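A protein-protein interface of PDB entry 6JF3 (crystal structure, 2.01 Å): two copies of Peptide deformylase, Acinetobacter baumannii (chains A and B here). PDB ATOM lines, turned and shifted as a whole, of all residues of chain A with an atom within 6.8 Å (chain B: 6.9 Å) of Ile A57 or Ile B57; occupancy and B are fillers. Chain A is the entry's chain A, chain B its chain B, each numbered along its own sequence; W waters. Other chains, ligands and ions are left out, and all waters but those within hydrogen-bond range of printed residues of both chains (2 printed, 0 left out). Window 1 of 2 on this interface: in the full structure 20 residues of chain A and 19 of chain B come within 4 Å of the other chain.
The backbone carbonyl oxygen (O) of Tyr B56 is in hydrogen-bond range of the backbone NH (N) of Ser A58. O of Tyr A56 lies within hydrogen-bond range of N of Ser B58.
The backbone carbonyl oxygen of Ala A52 sits at hydrogen-bond distance from the backbone NH of Ile A57. O of Ala B52 lies within hydrogen-bond range of N of Ile B57, at 3.1 Å.
CD2 of Leu A4 touches NE1 of Trp B30 (3.5 Å). Ile A13 touches Ile B13 (CD1 to CD1, 3.8 Å). CB of Ser B58 touches CD1 of Ile A13, 3.9 Å away. CZ3 of Trp B30 touches CZ3 of Trp A30 (3.8 Å). Ile B57 touches Trp A30. O of Tyr A56 touches C of Ile B57, 3.8 Å away. Ile A57 touches Trp B30. Tyr B56 touches Ile A57. Ile A57 touches Ile B57 (CG2 to CD1, 3.6 Å). Ile B13 touches Ser A58 (CD1 to CB, 3.9 Å).
Printed residues of chain B within 4 Å of Leu A4: Trp B30 (3.5 Å). Printed residues of chain B within 4 Å of Trp A30: Leu B4 (3.4 Å), Trp B30 (3.8 Å) and Ile B57 (3.7 Å). Of the printed residues of chain B, Val A55 touches Lys B59 (3.8 Å). Ile A57 touches three residues of chain B. Arg A60 touches none of the printed residues of chain B. Ala B52 touches none of the printed residues of chain A. Ile B57 touches just these residues of chain A: Trp A30, Tyr A56 and Ile A57. The nearest residue of chain B that does not touch Ile A57 is Lys B59 (4.7 Å). The nearest printed residue of chain B that does not touch Tyr A56 is Tyr B56 (4.2 Å).
Of the 18 printed residues of chain A, 7 touch a printed residue of chain B. Hydrophobic or aromatic side chains of chain B that line the printed part of chain A: Leu B4, Ile B13, Trp B30, Tyr B56 and Ile B57. Among the printed residues, 14 pairs touch across the chains.
Ile A13 touches its own counterpart, Ile B13. Ile A13 touches Ser B58, and with the chains exchanged Ser A58 touches Ile B13. Tyr A56 touches Ile B57, and with the chains exchanged Ile A57 touches Tyr B56. Tyr A56 touches Ser B58, and with the chains exchanged Ser A58 touches Tyr B56. Of the 14 pairs that touch across the chains among the printed residues, 13 have their exchanged pair printed and touching as well.
Water W2 bridges NZ of Lys A59 (2.8 Å) and O of Val B55 (2.9 Å). Water W1 bridges the side-chain amino group of Lys B59 (2.8 Å) and the backbone carbonyl oxygen of Val A55 (2.8 Å).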
ATOM      1  N   LEU A   4      -2.968   6.533 -23.147  1.00  0.00           N
ATOM      2  CA  LEU A   4      -4.357   6.637 -22.700  1.00  0.00           C
ATOM      3  C   LEU A   4      -4.620   5.693 -21.517  1.00  0.00           C
ATOM      4  O   LEU A   4      -3.951   4.669 -21.378  1.00  0.00           O
ATOM      5  CB  LEU A   4      -5.317   6.280 -23.852  1.00  0.00           C
ATOM      6  CG  LEU A   4      -5.351   7.145 -25.113  1.00  0.00           C
ATOM      7  CD1 LEU A   4      -6.261   6.557 -26.205  1.00  0.00           C
ATOM      8  CD2 LEU A   4      -5.822   8.548 -24.767  1.00  0.00           C
ATOM      9  N   ILE A  13     -17.770  -1.100 -20.237  1.00  0.00           N
ATOM     10  CA  ILE A  13     -17.352  -0.682 -21.591  1.00  0.00           C
ATOM     11  C   ILE A  13     -16.821  -1.864 -22.394  1.00  0.00           C
ATOM     12  O   ILE A  13     -17.093  -1.999 -23.586  1.00  0.00           O
ATOM     13  CB  ILE A  13     -16.319   0.481 -21.538  1.00  0.00           C
ATOM     14  CG1 ILE A  13     -15.964   1.041 -22.922  1.00  0.00           C
ATOM     15  CG2 ILE A  13     -15.001   0.074 -20.835  1.00  0.00           C
ATOM     16  CD1 ILE A  13     -17.071   1.662 -23.686  1.00  0.00           C
ATOM     17  N   ALA A  18     -19.002  -2.824 -29.959  1.00  0.00           N
ATOM     18  CA  ALA A  18     -18.506  -1.537 -30.387  1.00  0.00           C
ATOM     19  C   ALA A  18     -19.124  -1.148 -31.676  1.00  0.00           C
ATOM     20  O   ALA A  18     -19.322  -1.982 -32.510  1.00  0.00           O
ATOM     21  CB  ALA A  18     -16.987  -1.602 -30.566  1.00  0.00           C
ATOM     22  N   TRP A  30      -9.258  13.007 -36.814  1.00  0.00           N
ATOM     23  CA  TRP A  30      -9.886  12.287 -35.704  1.00  0.00           C
ATOM     24  C   TRP A  30      -9.380  10.839 -35.589  1.00  0.00           C
ATOM     25  O   TRP A  30      -8.794  10.443 -34.577  1.00  0.00           O
ATOM     26  CB  TRP A  30     -11.431  12.418 -35.835  1.00  0.00           C
ATOM     27  CG  TRP A  30     -12.236  11.298 -35.265  1.00  0.00           C
ATOM     28  CD1 TRP A  30     -12.955  10.389 -35.958  1.00  0.00           C
ATOM     29  CD2 TRP A  30     -12.379  10.964 -33.904  1.00  0.00           C
ATOM     30  NE1 TRP A  30     -13.557   9.508 -35.119  1.00  0.00           N
ATOM     31  CE2 TRP A  30     -13.229   9.837 -33.840  1.00  0.00           C
ATOM     32  CE3 TRP A  30     -11.899  11.515 -32.727  1.00  0.00           C
ATOM     33  CZ2 TRP A  30     -13.587   9.226 -32.640  1.00  0.00           C
ATOM     34  CZ3 TRP A  30     -12.249  10.920 -31.532  1.00  0.00           C
ATOM     35  CH2 TRP A  30     -13.081   9.782 -31.496  1.00  0.00           C
ATOM     36  N   LEU A  34      -6.822   8.975 -33.065  1.00  0.00           N
ATOM     37  CA  LEU A  34      -7.293   7.823 -32.244  1.00  0.00           C
ATOM     38  C   LEU A  34      -6.318   6.674 -32.396  1.00  0.00           C
ATOM     39  O   LEU A  34      -5.827   6.093 -31.417  1.00  0.00           O
ATOM     40  CB  LEU A  34      -8.698   7.397 -32.676  1.00  0.00           C
ATOM     41  CG  LEU A  34      -9.202   6.022 -32.204  1.00  0.00           C
ATOM     42  CD1 LEU A  34      -9.223   5.949 -30.687  1.00  0.00           C
ATOM     43  CD2 LEU A  34     -10.593   5.816 -32.726  1.00  0.00           C
ATOM     44  N   MET A  38      -3.929   4.936 -29.495  1.00  0.00           N
ATOM     45  CA  MET A  38      -4.029   3.511 -29.245  1.00  0.00           C
ATOM     46  C   MET A  38      -2.669   2.840 -29.423  1.00  0.00           C
ATOM     47  O   MET A  38      -2.277   1.976 -28.608  1.00  0.00           O
ATOM     48  CB  MET A  38      -5.055   2.824 -30.136  1.00  0.00           C
ATOM     49  CG  MET A  38      -6.487   3.182 -29.789  1.00  0.00           C
ATOM     50  SD  MET A  38      -7.576   2.519 -31.112  1.00  0.00           S
ATOM     51  CE  MET A  38      -7.209   0.768 -30.996  1.00  0.00           C
ATOM     52  N   ALA A  51      -7.551  -3.011 -28.723  1.00  0.00           N
ATOM     53  CA  ALA A  51      -8.825  -2.673 -29.305  1.00  0.00           C
ATOM     54  C   ALA A  51      -9.345  -1.356 -28.683  1.00  0.00           C
ATOM     55  O   ALA A  51      -9.169  -1.065 -27.486  1.00  0.00           O
ATOM     56  CB  ALA A  51      -9.767  -3.831 -29.083  1.00  0.00           C
ATOM     57  N   ALA A  52     -10.039  -0.561 -29.479  1.00  0.00           N
ATOM     58  CA  ALA A  52     -10.513   0.748 -29.006  1.00  0.00           C
ATOM     59  C   ALA A  52     -11.334   0.709 -27.677  1.00  0.00           C
ATOM     60  O   ALA A  52     -11.132   1.570 -26.791  1.00  0.00           O
ATOM     61  CB  ALA A  52     -11.244   1.466 -30.120  1.00  0.00           C
ATOM     62  N   PRO A  53     -12.207  -0.311 -27.505  1.00  0.00           N
ATOM     63  CA  PRO A  53     -12.899  -0.401 -26.199  1.00  0.00           C
ATOM     64  C   PRO A  53     -11.999  -0.413 -24.965  1.00  0.00           C
ATOM     65  O   PRO A  53     -12.432   0.066 -23.938  1.00  0.00           O
ATOM     66  CB  PRO A  53     -13.706  -1.662 -26.310  1.00  0.00           C
ATOM     67  CG  PRO A  53     -14.026  -1.764 -27.812  1.00  0.00           C
ATOM     68  CD  PRO A  53     -12.721  -1.310 -28.463  1.00  0.00           C
ATOM     69  N   GLN A  54     -10.772  -0.897 -25.070  1.00  0.00           N
ATOM     70  CA  GLN A  54      -9.853  -0.903 -23.979  1.00  0.00           C
ATOM     71  C   GLN A  54      -9.393   0.464 -23.578  1.00  0.00           C
ATOM     72  O   GLN A  54      -8.998   0.643 -22.452  1.00  0.00           O
ATOM     73  CB  GLN A  54      -8.630  -1.769 -24.326  1.00  0.00           C
ATOM     74  CG  GLN A  54      -8.959  -3.225 -24.487  1.00  0.00           C
ATOM     75  CD  GLN A  54      -7.748  -4.053 -24.791  1.00  0.00           C
ATOM     76  OE1 GLN A  54      -7.270  -4.065 -25.948  1.00  0.00           O
ATOM     77  NE2 GLN A  54      -7.237  -4.768 -23.765  1.00  0.00           N
ATOM     78  N   VAL A  55      -9.495   1.447 -24.468  1.00  0.00           N
ATOM     79  CA  VAL A  55      -9.221   2.844 -24.119  1.00  0.00           C
ATOM     80  C   VAL A  55     -10.519   3.677 -24.087  1.00  0.00           C
ATOM     81  O   VAL A  55     -10.502   4.920 -24.294  1.00  0.00           O
ATOM     82  CB  VAL A  55      -8.150   3.463 -25.011  1.00  0.00           C
ATOM     83  CG1 VAL A  55      -6.862   2.728 -24.813  1.00  0.00           C
ATOM     84  CG2 VAL A  55      -8.555   3.446 -26.484  1.00  0.00           C
ATOM     85  N   TYR A  56     -11.636   2.999 -23.754  1.00  0.00           N
ATOM     86  CA  TYR A  56     -12.951   3.638 -23.569  1.00  0.00           C
ATOM     87  C   TYR A  56     -13.580   4.202 -24.826  1.00  0.00           C
ATOM     88  O   TYR A  56     -14.475   5.091 -24.755  1.00  0.00           O
ATOM     89  CB  TYR A  56     -12.874   4.694 -22.456  1.00  0.00           C
ATOM     90  CG  TYR A  56     -12.430   4.167 -21.100  1.00  0.00           C
ATOM     91  CD1 TYR A  56     -13.343   3.562 -20.250  1.00  0.00           C
ATOM     92  CD2 TYR A  56     -11.127   4.256 -20.690  1.00  0.00           C
ATOM     93  CE1 TYR A  56     -12.978   3.054 -19.032  1.00  0.00           C
ATOM     94  CE2 TYR A  56     -10.727   3.756 -19.438  1.00  0.00           C
ATOM     95  CZ  TYR A  56     -11.664   3.146 -18.640  1.00  0.00           C
ATOM     96  OH  TYR A  56     -11.278   2.678 -17.417  1.00  0.00           O
ATOM     97  N   ILE A  57     -13.146   3.718 -26.004  1.00  0.00           N
ATOM     98  CA  ILE A  57     -13.715   4.207 -27.249  1.00  0.00           C
ATOM     99  C   ILE A  57     -14.498   3.047 -27.809  1.00  0.00           C
ATOM    100  O   ILE A  57     -13.896   2.056 -28.218  1.00  0.00           O
ATOM    101  CB  ILE A  57     -12.646   4.618 -28.247  1.00  0.00           C
ATOM    102  CG1 ILE A  57     -11.638   5.626 -27.615  1.00  0.00           C
ATOM    103  CG2 ILE A  57     -13.303   5.144 -29.516  1.00  0.00           C
ATOM    104  CD1 ILE A  57     -12.126   6.958 -27.108  1.00  0.00           C
ATOM    105  N   SER A  58     -15.828   3.147 -27.824  1.00  0.00           N
ATOM    106  CA  SER A  58     -16.633   2.013 -28.263  1.00  0.00           C
ATOM    107  C   SER A  58     -16.783   2.020 -29.796  1.00  0.00           C
ATOM    108  O   SER A  58     -17.887   2.135 -30.332  1.00  0.00           O
ATOM    109  CB  SER A  58     -17.984   1.978 -27.556  1.00  0.00           C
ATOM    110  OG  SER A  58     -18.549   0.673 -27.653  1.00  0.00           O
ATOM    111  N   LYS A  59     -15.663   1.840 -30.478  1.00  0.00           N
ATOM    112  CA  LYS A  59     -15.583   1.874 -31.917  1.00  0.00           C
ATOM    113  C   LYS A  59     -14.770   0.671 -32.389  1.00  0.00           C
ATOM    114  O   LYS A  59     -13.847   0.222 -31.700  1.00  0.00           O
ATOM    115  CB  LYS A  59     -14.857   3.137 -32.359  1.00  0.00           C
ATOM    116  CG  LYS A  59     -15.597   4.419 -32.136  1.00  0.00           C
ATOM    117  CD  LYS A  59     -16.738   4.654 -33.118  1.00  0.00           C
ATOM    118  CE  LYS A  59     -16.953   6.147 -33.331  1.00  0.00           C
ATOM    119  NZ  LYS A  59     -17.925   6.279 -34.415  1.00  0.00           N
ATOM    120  N   ARG A  60     -15.044   0.217 -33.602  1.00  0.00           N
ATOM    121  CA  ARG A  60     -14.414  -0.987 -34.190  1.00  0.00           C
ATOM    122  C   ARG A  60     -13.058  -0.677 -34.863  1.00  0.00           C
ATOM    123  O   ARG A  60     -12.951  -0.611 -36.097  1.00  0.00           O
ATOM    124  CB  ARG A  60     -15.368  -1.663 -35.146  1.00  0.00           C
ATOM    125  CG  ARG A  60     -16.698  -2.048 -34.501  1.00  0.00           C
ATOM    126  CD  ARG A  60     -17.616  -2.900 -35.377  1.00  0.00           C
ATOM    127  NE  ARG A  60     -17.212  -4.300 -35.272  1.00  0.00           N
ATOM    128  CZ  ARG A  60     -17.473  -5.101 -34.248  1.00  0.00           C
ATOM    129  NH1 ARG A  60     -18.136  -4.649 -33.198  1.00  0.00           N
ATOM    130  NH2 ARG A  60     -17.009  -6.348 -34.227  1.00  0.00           N
ATOM    131  N   VAL A  61     -12.056  -0.427 -34.023  1.00  0.00           N
ATOM    132  CA  VAL A  61     -10.694  -0.211 -34.446  1.00  0.00           C
ATOM    133  C   VAL A  61      -9.795  -1.075 -33.576  1.00  0.00           C
ATOM    134  O   VAL A  61      -9.926  -1.054 -32.338  1.00  0.00           O
ATOM    135  CB  VAL A  61     -10.277   1.245 -34.246  1.00  0.00           C
ATOM    136  CG1 VAL A  61      -8.843   1.479 -34.762  1.00  0.00           C
ATOM    137  CG2 VAL A  61     -11.243   2.139 -34.990  1.00  0.00           C
ATOM    138  N   LEU A 149     -14.074  -6.153 -29.477  1.00  0.00           N
ATOM    139  CA  LEU A 149     -15.103  -5.382 -30.202  1.00  0.00           C
ATOM    140  C   LEU A 149     -16.506  -5.919 -30.043  1.00  0.00           C
ATOM    141  O   LEU A 149     -17.448  -5.199 -30.247  1.00  0.00           O
ATOM    142  CB  LEU A 149     -14.836  -5.304 -31.702  1.00  0.00           C
ATOM    143  CG  LEU A 149     -13.461  -4.736 -32.096  1.00  0.00           C
ATOM    144  CD1 LEU A 149     -13.337  -4.606 -33.593  1.00  0.00           C
ATOM    145  CD2 LEU A 149     -13.209  -3.391 -31.418  1.00  0.00           C
ATOM    146  N   LEU B   4     -19.664  12.919 -35.946  1.00  0.00           N
ATOM    147  CA  LEU B   4     -19.683  11.542 -35.444  1.00  0.00           C
ATOM    148  C   LEU B   4     -21.100  10.912 -35.389  1.00  0.00           C
ATOM    149  O   LEU B   4     -22.071  11.622 -35.189  1.00  0.00           O
ATOM    150  CB  LEU B   4     -19.013  11.483 -34.071  1.00  0.00           C
ATOM    151  CG  LEU B   4     -17.526  11.886 -34.003  1.00  0.00           C
ATOM    152  CD1 LEU B   4     -16.994  12.059 -32.574  1.00  0.00           C
ATOM    153  CD2 LEU B   4     -16.712  10.827 -34.742  1.00  0.00           C
ATOM    154  N   ILE B  13     -23.959   1.889 -24.386  1.00  0.00           N
ATOM    155  CA  ILE B  13     -22.952   2.952 -24.171  1.00  0.00           C
ATOM    156  C   ILE B  13     -23.504   4.139 -23.357  1.00  0.00           C
ATOM    157  O   ILE B  13     -22.796   4.738 -22.557  1.00  0.00           O
ATOM    158  CB  ILE B  13     -22.413   3.470 -25.538  1.00  0.00           C
ATOM    159  CG1 ILE B  13     -21.245   4.426 -25.402  1.00  0.00           C
ATOM    160  CG2 ILE B  13     -23.514   4.148 -26.323  1.00  0.00           C
ATOM    161  CD1 ILE B  13     -19.987   3.840 -24.804  1.00  0.00           C
ATOM    162  N   ALA B  18     -19.043   7.182 -17.382  1.00  0.00           N
ATOM    163  CA  ALA B  18     -17.920   7.535 -18.252  1.00  0.00           C
ATOM    164  C   ALA B  18     -16.658   7.718 -17.413  1.00  0.00           C
ATOM    165  O   ALA B  18     -16.743   8.139 -16.264  1.00  0.00           O
ATOM    166  CB  ALA B  18     -18.237   8.795 -19.011  1.00  0.00           C
ATOM    167  N   TRP B  30      -4.899  14.652 -29.610  1.00  0.00           N
ATOM    168  CA  TRP B  30      -5.929  13.673 -29.351  1.00  0.00           C
ATOM    169  C   TRP B  30      -7.200  14.373 -28.835  1.00  0.00           C
ATOM    170  O   TRP B  30      -8.263  14.333 -29.477  1.00  0.00           O
ATOM    171  CB  TRP B  30      -5.382  12.614 -28.377  1.00  0.00           C
ATOM    172  CG  TRP B  30      -6.435  11.964 -27.580  1.00  0.00           C
ATOM    173  CD1 TRP B  30      -6.583  12.004 -26.217  1.00  0.00           C
ATOM    174  CD2 TRP B  30      -7.532  11.221 -28.086  1.00  0.00           C
ATOM    175  NE1 TRP B  30      -7.720  11.326 -25.847  1.00  0.00           N
ATOM    176  CE2 TRP B  30      -8.318  10.820 -26.970  1.00  0.00           C
ATOM    177  CE3 TRP B  30      -7.946  10.868 -29.380  1.00  0.00           C
ATOM    178  CZ2 TRP B  30      -9.512  10.089 -27.107  1.00  0.00           C
ATOM    179  CZ3 TRP B  30      -9.137  10.118 -29.527  1.00  0.00           C
ATOM    180  CH2 TRP B  30      -9.905   9.739 -28.388  1.00  0.00           C
ATOM    181  N   LEU B  34     -10.928  15.222 -30.538  1.00  0.00           N
ATOM    182  CA  LEU B  34     -12.192  14.752 -29.943  1.00  0.00           C
ATOM    183  C   LEU B  34     -13.216  15.901 -29.759  1.00  0.00           C
ATOM    184  O   LEU B  34     -14.375  15.827 -30.196  1.00  0.00           O
ATOM    185  CB  LEU B  34     -11.933  14.085 -28.562  1.00  0.00           C
ATOM    186  CG  LEU B  34     -13.171  13.814 -27.672  1.00  0.00           C
ATOM    187  CD1 LEU B  34     -14.099  12.844 -28.384  1.00  0.00           C
ATOM    188  CD2 LEU B  34     -12.781  13.249 -26.327  1.00  0.00           C
ATOM    189  N   MET B  38     -16.834  16.416 -31.587  1.00  0.00           N
ATOM    190  CA  MET B  38     -18.037  16.608 -30.770  1.00  0.00           C
ATOM    191  C   MET B  38     -18.724  17.943 -31.095  1.00  0.00           C
ATOM    192  O   MET B  38     -19.937  17.983 -31.229  1.00  0.00           O
ATOM    193  CB  MET B  38     -17.701  16.572 -29.273  1.00  0.00           C
ATOM    194  CG  MET B  38     -17.248  15.191 -28.756  1.00  0.00           C
ATOM    195  SD  MET B  38     -16.744  15.207 -27.006  1.00  0.00           S
ATOM    196  CE  MET B  38     -18.239  15.861 -26.235  1.00  0.00           C
ATOM    197  N   ALA B  51     -22.482  15.412 -25.053  1.00  0.00           N
ATOM    198  CA  ALA B  51     -21.611  14.664 -24.140  1.00  0.00           C
ATOM    199  C   ALA B  51     -20.958  13.503 -24.913  1.00  0.00           C
ATOM    200  O   ALA B  51     -21.579  12.900 -25.770  1.00  0.00           O
ATOM    201  CB  ALA B  51     -22.385  14.187 -22.933  1.00  0.00           C
ATOM    202  N   ALA B  52     -19.703  13.223 -24.595  1.00  0.00           N
ATOM    203  CA  ALA B  52     -18.940  12.193 -25.265  1.00  0.00           C
ATOM    204  C   ALA B  52     -19.581  10.806 -25.390  1.00  0.00           C
ATOM    205  O   ALA B  52     -19.558  10.207 -26.497  1.00  0.00           O
ATOM    206  CB  ALA B  52     -17.532  12.122 -24.698  1.00  0.00           C
ATOM    207  N   PRO B  53     -20.185  10.275 -24.296  1.00  0.00           N
ATOM    208  CA  PRO B  53     -20.928   8.997 -24.483  1.00  0.00           C
ATOM    209  C   PRO B  53     -21.875   8.932 -25.693  1.00  0.00           C
ATOM    210  O   PRO B  53     -22.052   7.856 -26.301  1.00  0.00           O
ATOM    211  CB  PRO B  53     -21.653   8.853 -23.143  1.00  0.00           C
ATOM    212  CG  PRO B  53     -20.647   9.461 -22.171  1.00  0.00           C
ATOM    213  CD  PRO B  53     -20.114  10.652 -22.869  1.00  0.00           C
ATOM    214  N   GLN B  54     -22.451  10.069 -26.072  1.00  0.00           N
ATOM    215  CA  GLN B  54     -23.395  10.089 -27.144  1.00  0.00           C
ATOM    216  C   GLN B  54     -22.742   9.888 -28.492  1.00  0.00           C
ATOM    217  O   GLN B  54     -23.453   9.510 -29.426  1.00  0.00           O
ATOM    218  CB  GLN B  54     -24.214  11.382 -27.170  1.00  0.00           C
ATOM    219  CG  GLN B  54     -25.026  11.717 -25.936  1.00  0.00           C
ATOM    220  CD  GLN B  54     -25.630  13.126 -26.046  1.00  0.00           C
ATOM    221  OE1 GLN B  54     -24.946  14.156 -25.769  1.00  0.00           O
ATOM    222  NE2 GLN B  54     -26.881  13.186 -26.523  1.00  0.00           N
ATOM    223  N   VAL B  55     -21.425  10.080 -28.606  1.00  0.00           N
ATOM    224  CA  VAL B  55     -20.690   9.736 -29.846  1.00  0.00           C
ATOM    225  C   VAL B  55     -19.758   8.507 -29.654  1.00  0.00           C
ATOM    226  O   VAL B  55     -18.695   8.399 -30.244  1.00  0.00           O
ATOM    227  CB  VAL B  55     -19.935  10.988 -30.419  1.00  0.00           C
ATOM    228  CG1 VAL B  55     -20.925  12.066 -30.778  1.00  0.00           C
ATOM    229  CG2 VAL B  55     -18.922  11.569 -29.423  1.00  0.00           C
ATOM    230  N   TYR B  56     -20.183   7.600 -28.774  1.00  0.00           N
ATOM    231  CA  TYR B  56     -19.511   6.371 -28.421  1.00  0.00           C
ATOM    232  C   TYR B  56     -18.147   6.516 -27.748  1.00  0.00           C
ATOM    233  O   TYR B  56     -17.304   5.633 -27.820  1.00  0.00           O
ATOM    234  CB  TYR B  56     -19.444   5.403 -29.596  1.00  0.00           C
ATOM    235  CG  TYR B  56     -20.781   5.013 -30.161  1.00  0.00           C
ATOM    236  CD1 TYR B  56     -21.360   5.763 -31.199  1.00  0.00           C
ATOM    237  CD2 TYR B  56     -21.471   3.906 -29.677  1.00  0.00           C
ATOM    238  CE1 TYR B  56     -22.585   5.452 -31.743  1.00  0.00           C
ATOM    239  CE2 TYR B  56     -22.723   3.601 -30.187  1.00  0.00           C
ATOM    240  CZ  TYR B  56     -23.257   4.387 -31.221  1.00  0.00           C
ATOM    241  OH  TYR B  56     -24.457   4.101 -31.784  1.00  0.00           O
ATOM    242  N   ILE B  57     -17.929   7.618 -27.064  1.00  0.00           N
ATOM    243  CA  ILE B  57     -16.681   7.829 -26.375  1.00  0.00           C
ATOM    244  C   ILE B  57     -17.033   7.860 -24.907  1.00  0.00           C
ATOM    245  O   ILE B  57     -17.659   8.818 -24.433  1.00  0.00           O
ATOM    246  CB  ILE B  57     -16.071   9.158 -26.791  1.00  0.00           C
ATOM    247  CG1 ILE B  57     -15.904   9.292 -28.312  1.00  0.00           C
ATOM    248  CG2 ILE B  57     -14.747   9.410 -26.081  1.00  0.00           C
ATOM    249  CD1 ILE B  57     -15.198   8.194 -28.971  1.00  0.00           C
ATOM    250  N   SER B  58     -16.622   6.851 -24.158  1.00  0.00           N
ATOM    251  CA  SER B  58     -17.021   6.760 -22.738  1.00  0.00           C
ATOM    252  C   SER B  58     -16.007   7.517 -21.832  1.00  0.00           C
ATOM    253  O   SER B  58     -15.319   6.924 -20.994  1.00  0.00           O
ATOM    254  CB  SER B  58     -17.164   5.286 -22.309  1.00  0.00           C
ATOM    255  OG  SER B  58     -18.017   5.244 -21.184  1.00  0.00           O
ATOM    256  N   LYS B  59     -15.975   8.833 -22.023  1.00  0.00           N
ATOM    257  CA  LYS B  59     -15.071   9.765 -21.377  1.00  0.00           C
ATOM    258  C   LYS B  59     -15.845  10.996 -20.932  1.00  0.00           C
ATOM    259  O   LYS B  59     -16.851  11.398 -21.553  1.00  0.00           O
ATOM    260  CB  LYS B  59     -13.971  10.161 -22.339  1.00  0.00           C
ATOM    261  CG  LYS B  59     -13.026   9.004 -22.611  1.00  0.00           C
ATOM    262  CD  LYS B  59     -11.649   9.518 -22.936  1.00  0.00           C
ATOM    263  CE  LYS B  59     -10.594   8.423 -22.885  1.00  0.00           C
ATOM    264  NZ  LYS B  59      -9.751   8.529 -21.679  1.00  0.00           N
ATOM    265  N   ARG B  60     -15.376  11.597 -19.854  1.00  0.00           N
ATOM    266  CA  ARG B  60     -16.062  12.695 -19.191  1.00  0.00           C
ATOM    267  C   ARG B  60     -15.704  14.000 -19.874  1.00  0.00           C
ATOM    268  O   ARG B  60     -14.914  14.780 -19.355  1.00  0.00           O
ATOM    269  CB  ARG B  60     -15.707  12.702 -17.694  1.00  0.00           C
ATOM    270  CG  ARG B  60     -16.184  11.420 -17.018  1.00  0.00           C
ATOM    271  CD  ARG B  60     -16.035  11.401 -15.499  1.00  0.00           C
ATOM    272  NE  ARG B  60     -17.236  11.982 -14.860  1.00  0.00           N
ATOM    273  CZ  ARG B  60     -18.399  11.349 -14.674  1.00  0.00           C
ATOM    274  NH1 ARG B  60     -18.616  10.092 -15.084  1.00  0.00           N
ATOM    275  NH2 ARG B  60     -19.378  12.003 -14.091  1.00  0.00           N
ATOM    276  N   VAL B  61     -16.289  14.218 -21.057  1.00  0.00           N
ATOM    277  CA  VAL B  61     -16.128  15.473 -21.814  1.00  0.00           C
ATOM    278  C   VAL B  61     -17.507  15.906 -22.232  1.00  0.00           C
ATOM    279  O   VAL B  61     -18.311  15.096 -22.757  1.00  0.00           O
ATOM    280  CB  VAL B  61     -15.284  15.300 -23.086  1.00  0.00           C
ATOM    281  CG1 VAL B  61     -15.033  16.647 -23.783  1.00  0.00           C
ATOM    282  CG2 VAL B  61     -13.976  14.693 -22.726  1.00  0.00           C
ATOM    283  N   LEU B 149     -22.845  11.601 -18.552  1.00  0.00           N
ATOM    284  CA  LEU B 149     -21.655  11.031 -17.992  1.00  0.00           C
ATOM    285  C   LEU B 149     -21.917   9.996 -16.915  1.00  0.00           C
ATOM    286  O   LEU B 149     -21.043   9.203 -16.683  1.00  0.00           O
ATOM    287  CB  LEU B 149     -20.720  12.080 -17.437  1.00  0.00           C
ATOM    288  CG  LEU B 149     -20.360  13.206 -18.366  1.00  0.00           C
ATOM    289  CD1 LEU B 149     -19.359  14.149 -17.727  1.00  0.00           C
ATOM    290  CD2 LEU B 149     -19.842  12.648 -19.686  1.00  0.00           C
HETATM  291  O   HOH W   1      -8.593   6.096 -22.557  1.00  0.00           O
HETATM  292  O   HOH W   2     -19.463   8.191 -33.021  1.00  0.00           O
